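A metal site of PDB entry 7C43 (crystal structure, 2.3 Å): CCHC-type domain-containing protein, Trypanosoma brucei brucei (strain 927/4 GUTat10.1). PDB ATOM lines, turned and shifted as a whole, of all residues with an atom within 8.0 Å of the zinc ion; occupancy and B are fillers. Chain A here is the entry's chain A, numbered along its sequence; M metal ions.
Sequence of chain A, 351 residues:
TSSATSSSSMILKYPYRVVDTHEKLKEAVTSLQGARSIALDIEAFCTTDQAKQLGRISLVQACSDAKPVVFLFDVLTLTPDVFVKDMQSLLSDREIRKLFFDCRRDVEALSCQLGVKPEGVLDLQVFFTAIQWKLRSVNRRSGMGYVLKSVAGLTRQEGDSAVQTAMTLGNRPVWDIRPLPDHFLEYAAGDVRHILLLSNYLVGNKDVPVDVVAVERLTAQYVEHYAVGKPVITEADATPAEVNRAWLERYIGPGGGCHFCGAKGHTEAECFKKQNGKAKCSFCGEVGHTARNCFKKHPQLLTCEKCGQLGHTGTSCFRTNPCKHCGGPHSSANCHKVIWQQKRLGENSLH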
ATOM      1  N   LYS A 280     -14.207 -27.361  21.441  1.00  0.00           N
ATOM      2  CA  LYS A 280     -14.458 -27.994  22.736  1.00  0.00           C
ATOM      3  C   LYS A 280     -13.119 -27.927  23.499  1.00  0.00           C
ATOM      4  O   LYS A 280     -12.077 -28.292  22.925  1.00  0.00           O
ATOM      5  CB  LYS A 280     -14.856 -29.467  22.504  1.00  0.00           C
ATOM      6  CG  LYS A 280     -15.693 -30.158  23.584  1.00  0.00           C
ATOM      7  CD  LYS A 280     -15.768 -31.672  23.288  1.00  0.00           C
ATOM      8  CE  LYS A 280     -17.053 -32.323  23.758  1.00  0.00           C
ATOM      9  NZ  LYS A 280     -17.349 -32.034  25.187  1.00  0.00           N
ATOM     10  N   CYS A 281     -13.128 -27.460  24.749  1.00  0.00           N
ATOM     11  CA  CYS A 281     -11.877 -27.367  25.514  1.00  0.00           C
ATOM     12  C   CYS A 281     -11.369 -28.747  25.954  1.00  0.00           C
ATOM     13  O   CYS A 281     -12.048 -29.429  26.710  1.00  0.00           O
ATOM     14  CB  CYS A 281     -12.043 -26.499  26.757  1.00  0.00           C
ATOM     15  SG  CYS A 281     -10.449 -26.154  27.520  1.00  0.00           S
ATOM     16  N   SER A 282     -10.163 -29.132  25.506  1.00  0.00           N
ATOM     17  CA  SER A 282      -9.567 -30.416  25.915  1.00  0.00           C
ATOM     18  C   SER A 282      -9.312 -30.511  27.437  1.00  0.00           C
ATOM     19  O   SER A 282      -9.437 -31.585  28.017  1.00  0.00           O
ATOM     20  CB  SER A 282      -8.275 -30.737  25.114  1.00  0.00           C
ATOM     21  OG  SER A 282      -7.285 -29.726  25.204  1.00  0.00           O
ATOM     22  N   PHE A 283      -9.031 -29.389  28.076  1.00  0.00           N
ATOM     23  CA  PHE A 283      -8.814 -29.369  29.511  1.00  0.00           C
ATOM     24  C   PHE A 283     -10.086 -29.405  30.374  1.00  0.00           C
ATOM     25  O   PHE A 283     -10.195 -30.260  31.242  1.00  0.00           O
ATOM     26  CB  PHE A 283      -7.991 -28.154  29.886  1.00  0.00           C
ATOM     27  CG  PHE A 283      -7.499 -28.186  31.304  1.00  0.00           C
ATOM     28  CD1 PHE A 283      -6.388 -28.979  31.656  1.00  0.00           C
ATOM     29  CD2 PHE A 283      -8.151 -27.453  32.295  1.00  0.00           C
ATOM     30  CE1 PHE A 283      -5.935 -29.012  32.957  1.00  0.00           C
ATOM     31  CE2 PHE A 283      -7.691 -27.491  33.591  1.00  0.00           C
ATOM     32  CZ  PHE A 283      -6.589 -28.280  33.923  1.00  0.00           C
ATOM     33  N   CYS A 284     -11.014 -28.459  30.187  1.00  0.00           N
ATOM     34  CA  CYS A 284     -12.247 -28.403  31.035  1.00  0.00           C
ATOM     35  C   CYS A 284     -13.526 -28.983  30.407  1.00  0.00           C
ATOM     36  O   CYS A 284     -14.548 -29.089  31.088  1.00  0.00           O
ATOM     37  CB  CYS A 284     -12.512 -26.968  31.508  1.00  0.00           C
ATOM     38  SG  CYS A 284     -13.296 -25.805  30.341  1.00  0.00           S
ATOM     39  N   GLY A 285     -13.488 -29.338  29.121  1.00  0.00           N
ATOM     40  CA  GLY A 285     -14.653 -29.866  28.442  1.00  0.00           C
ATOM     41  C   GLY A 285     -15.691 -28.884  27.895  1.00  0.00           C
ATOM     42  O   GLY A 285     -16.531 -29.298  27.111  1.00  0.00           O
ATOM     43  N   GLU A 286     -15.665 -27.610  28.277  1.00  0.00           N
ATOM     44  CA  GLU A 286     -16.721 -26.692  27.821  1.00  0.00           C
ATOM     45  C   GLU A 286     -16.550 -26.375  26.338  1.00  0.00           C
ATOM     46  O   GLU A 286     -15.414 -26.205  25.831  1.00  0.00           O
ATOM     47  CB  GLU A 286     -16.758 -25.402  28.642  1.00  0.00           C
ATOM     48  CG  GLU A 286     -17.137 -25.580  30.108  1.00  0.00           C
ATOM     49  CD  GLU A 286     -16.713 -24.390  30.969  1.00  0.00           C
ATOM     50  OE1 GLU A 286     -16.116 -24.582  32.053  1.00  0.00           O
ATOM     51  OE2 GLU A 286     -16.961 -23.231  30.547  1.00  0.00           O
ATOM     52  N   VAL A 287     -17.689 -26.360  25.643  1.00  0.00           N
ATOM     53  CA  VAL A 287     -17.776 -25.935  24.236  1.00  0.00           C
ATOM     54  C   VAL A 287     -17.693 -24.411  24.200  1.00  0.00           C
ATOM     55  O   VAL A 287     -18.331 -23.745  25.012  1.00  0.00           O
ATOM     56  CB  VAL A 287     -19.077 -26.456  23.542  1.00  0.00           C
ATOM     57  CG1 VAL A 287     -19.423 -25.702  22.248  1.00  0.00           C
ATOM     58  CG2 VAL A 287     -18.934 -27.958  23.242  1.00  0.00           C
ATOM     59  N   GLY A 288     -16.897 -23.877  23.285  1.00  0.00           N
ATOM     60  CA  GLY A 288     -16.745 -22.423  23.171  1.00  0.00           C
ATOM     61  C   GLY A 288     -15.340 -21.831  23.250  1.00  0.00           C
ATOM     62  O   GLY A 288     -15.130 -20.717  22.772  1.00  0.00           O
ATOM     63  N   HIS A 289     -14.386 -22.530  23.874  1.00  0.00           N
ATOM     64  CA  HIS A 289     -12.988 -22.118  23.800  1.00  0.00           C
ATOM     65  C   HIS A 289     -12.079 -23.296  23.594  1.00  0.00           C
ATOM     66  O   HIS A 289     -12.493 -24.431  23.708  1.00  0.00           O
ATOM     67  CB  HIS A 289     -12.575 -21.343  25.050  1.00  0.00           C
ATOM     68  CG  HIS A 289     -12.802 -22.073  26.338  1.00  0.00           C
ATOM     69  ND1 HIS A 289     -14.023 -22.067  26.982  1.00  0.00           N
ATOM     70  CD2 HIS A 289     -11.966 -22.804  27.123  1.00  0.00           C
ATOM     71  CE1 HIS A 289     -13.926 -22.754  28.107  1.00  0.00           C
ATOM     72  NE2 HIS A 289     -12.698 -23.210  28.211  1.00  0.00           N
ATOM     73  N   THR A 290     -10.843 -23.008  23.239  1.00  0.00           N
ATOM     74  CA  THR A 290      -9.824 -24.025  23.176  1.00  0.00           C
ATOM     75  C   THR A 290      -9.054 -24.023  24.501  1.00  0.00           C
ATOM     76  O   THR A 290      -9.140 -23.071  25.285  1.00  0.00           O
ATOM     77  CB  THR A 290      -8.836 -23.773  22.017  1.00  0.00           C
ATOM     78  OG1 THR A 290      -8.229 -22.483  22.178  1.00  0.00           O
ATOM     79  CG2 THR A 290      -9.526 -23.865  20.683  1.00  0.00           C
ATOM     80  N   ALA A 291      -8.276 -25.083  24.701  1.00  0.00           N
ATOM     81  CA  ALA A 291      -7.345 -25.196  25.836  1.00  0.00           C
ATOM     82  C   ALA A 291      -6.362 -24.047  25.934  1.00  0.00           C
ATOM     83  O   ALA A 291      -6.065 -23.561  27.041  1.00  0.00           O
ATOM     84  CB  ALA A 291      -6.572 -26.514  25.745  1.00  0.00           C
ATOM     85  N   ARG A 292      -5.828 -23.599  24.798  1.00  0.00           N
ATOM     86  CA  ARG A 292      -4.799 -22.574  24.821  1.00  0.00           C
ATOM     87  C   ARG A 292      -5.387 -21.249  25.305  1.00  0.00           C
ATOM     88  O   ARG A 292      -4.623 -20.394  25.726  1.00  0.00           O
ATOM     89  CB  ARG A 292      -4.055 -22.441  23.466  1.00  0.00           C
ATOM     90  CG  ARG A 292      -2.635 -21.880  23.656  1.00  0.00           C
ATOM     91  CD  ARG A 292      -1.708 -21.938  22.456  1.00  0.00           C
ATOM     92  NE  ARG A 292      -1.567 -23.302  21.911  1.00  0.00           N
ATOM     93  CZ  ARG A 292      -1.975 -23.714  20.708  1.00  0.00           C
ATOM     94  NH1 ARG A 292      -1.786 -24.992  20.359  1.00  0.00           N
ATOM     95  NH2 ARG A 292      -2.568 -22.889  19.838  1.00  0.00           N
ATOM     96  N   ASN A 293      -6.717 -21.121  25.295  1.00  0.00           N
ATOM     97  CA  ASN A 293      -7.454 -19.973  25.847  1.00  0.00           C
ATOM     98  C   ASN A 293      -8.236 -20.234  27.146  1.00  0.00           C
ATOM     99  O   ASN A 293      -9.064 -19.402  27.560  1.00  0.00           O
ATOM    100  CB  ASN A 293      -8.455 -19.454  24.785  1.00  0.00           C
ATOM    101  CG  ASN A 293      -7.759 -18.968  23.536  1.00  0.00           C
ATOM    102  OD1 ASN A 293      -8.061 -19.402  22.427  1.00  0.00           O
ATOM    103  ND2 ASN A 293      -6.788 -18.085  23.700  1.00  0.00           N
ATOM    104  N   CYS A 294      -7.953 -21.366  27.787  1.00  0.00           N
ATOM    105  CA  CYS A 294      -8.706 -21.813  28.959  1.00  0.00           C
ATOM    106  C   CYS A 294      -8.216 -21.146  30.238  1.00  0.00           C
ATOM    107  O   CYS A 294      -7.075 -21.353  30.649  1.00  0.00           O
ATOM    108  CB  CYS A 294      -8.655 -23.355  29.113  1.00  0.00           C
ATOM    109  SG  CYS A 294      -9.809 -24.006  30.363  1.00  0.00           S
ATOM    110  N   PHE A 295      -9.093 -20.325  30.841  1.00  0.00           N
ATOM    111  CA  PHE A 295      -8.847 -19.690  32.150  1.00  0.00           C
ATOM    112  C   PHE A 295      -8.442 -20.668  33.276  1.00  0.00           C
ATOM    113  O   PHE A 295      -7.612 -20.328  34.132  1.00  0.00           O
ATOM    114  CB  PHE A 295     -10.089 -18.901  32.616  1.00  0.00           C
ATOM    115  CG  PHE A 295     -10.450 -17.732  31.720  1.00  0.00           C
ATOM    116  CD1 PHE A 295      -9.524 -16.702  31.480  1.00  0.00           C
ATOM    117  CD2 PHE A 295     -11.720 -17.648  31.133  1.00  0.00           C
ATOM    118  CE1 PHE A 295      -9.859 -15.615  30.659  1.00  0.00           C
ATOM    119  CE2 PHE A 295     -12.047 -16.566  30.308  1.00  0.00           C
ATOM    120  CZ  PHE A 295     -11.113 -15.546  30.072  1.00  0.00           C
ATOM    121  N   LYS A 296      -9.023 -21.870  33.292  1.00  0.00           N
ATOM    122  CA  LYS A 296      -8.724 -22.886  34.296  1.00  0.00           C
ATOM    123  C   LYS A 296      -7.373 -23.558  34.051  1.00  0.00           C
ATOM    124  O   LYS A 296      -6.629 -23.772  34.996  1.00  0.00           O
ATOM    125  CB  LYS A 296      -9.819 -23.933  34.350  1.00  0.00           C
ATOM    126  CG  LYS A 296     -11.205 -23.380  34.653  1.00  0.00           C
ATOM    127  CD  LYS A 296     -12.159 -24.548  34.865  1.00  0.00           C
ATOM    128  CE  LYS A 296     -13.627 -24.188  34.735  1.00  0.00           C
ATOM    129  NZ  LYS A 296     -14.354 -24.368  36.033  1.00  0.00           N
ATOM    130  N   LYS A 297      -7.057 -23.893  32.808  1.00  0.00           N
ATOM    131  CA  LYS A 297      -5.727 -24.401  32.469  1.00  0.00           C
ATOM    132  C   LYS A 297      -4.645 -23.367  32.624  1.00  0.00           C
ATOM    133  O   LYS A 297      -3.545 -23.694  33.081  1.00  0.00           O
ATOM    134  CB  LYS A 297      -5.683 -24.927  31.044  1.00  0.00           C
ATOM    135  CG  LYS A 297      -4.376 -25.624  30.704  1.00  0.00           C
ATOM    136  CD  LYS A 297      -4.505 -26.563  29.518  1.00  0.00           C
ATOM    137  CE  LYS A 297      -3.137 -27.116  29.110  1.00  0.00           C
ATOM    138  NZ  LYS A 297      -3.173 -27.736  27.752  1.00  0.00           N
ATOM    139  N   HIS A 298      -4.922 -22.135  32.205  1.00  0.00           N
ATOM    140  CA  HIS A 298      -3.966 -21.018  32.273  1.00  0.00           C
ATOM    141  C   HIS A 298      -4.589 -19.846  33.045  1.00  0.00           C
ATOM    142  O   HIS A 298      -5.191 -18.975  32.435  1.00  0.00           O
ATOM    143  CB  HIS A 298      -3.587 -20.554  30.864  1.00  0.00           C
ATOM    144  CG  HIS A 298      -3.247 -21.669  29.920  1.00  0.00           C
ATOM    145  ND1 HIS A 298      -1.960 -22.120  29.720  1.00  0.00           N
ATOM    146  CD2 HIS A 298      -4.029 -22.375  29.070  1.00  0.00           C
ATOM    147  CE1 HIS A 298      -1.969 -23.091  28.814  1.00  0.00           C
ATOM    148  NE2 HIS A 298      -3.213 -23.250  28.401  1.00  0.00           N
HETATM  149 ZN    ZN M   1     -11.496 -24.876  29.240  1.00  0.00          ZN
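The side-chain sulfur (SG) of Cys 281 lies close to the backbone NH (N) of Ala 291 (3.7 Å).
The side-chain sulfur (SG) of Cys 281 lies close to the backbone NH (N) of Phe 283.
The side-chain carboxylate (OE1) of Glu 286 lies close to the side-chain sulfur (SG) of Cys 284.
The backbone NH (N) of Cys 281 sits at hydrogen-bond distance from the backbone carbonyl oxygen (O) of Glu 286, 2.8 Å away.
SG of Cys 294 lies close to N of Lys 297, at 3.7 Å.
SG of Cys 294 lies close to N of Lys 296 (3.7 Å).
SG of Cys 294 binds the zinc ion.
The zinc ion is bound by a ring nitrogen (NE2) of His 289 (2.3 Å).
The zinc ion is bound by the side-chain sulfur (SG) of Cys 284 (2.3 Å).
The zinc ion is bound by the side-chain sulfur (SG) of Cys 281.
The zinc ion has four donor atoms within binding distance.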
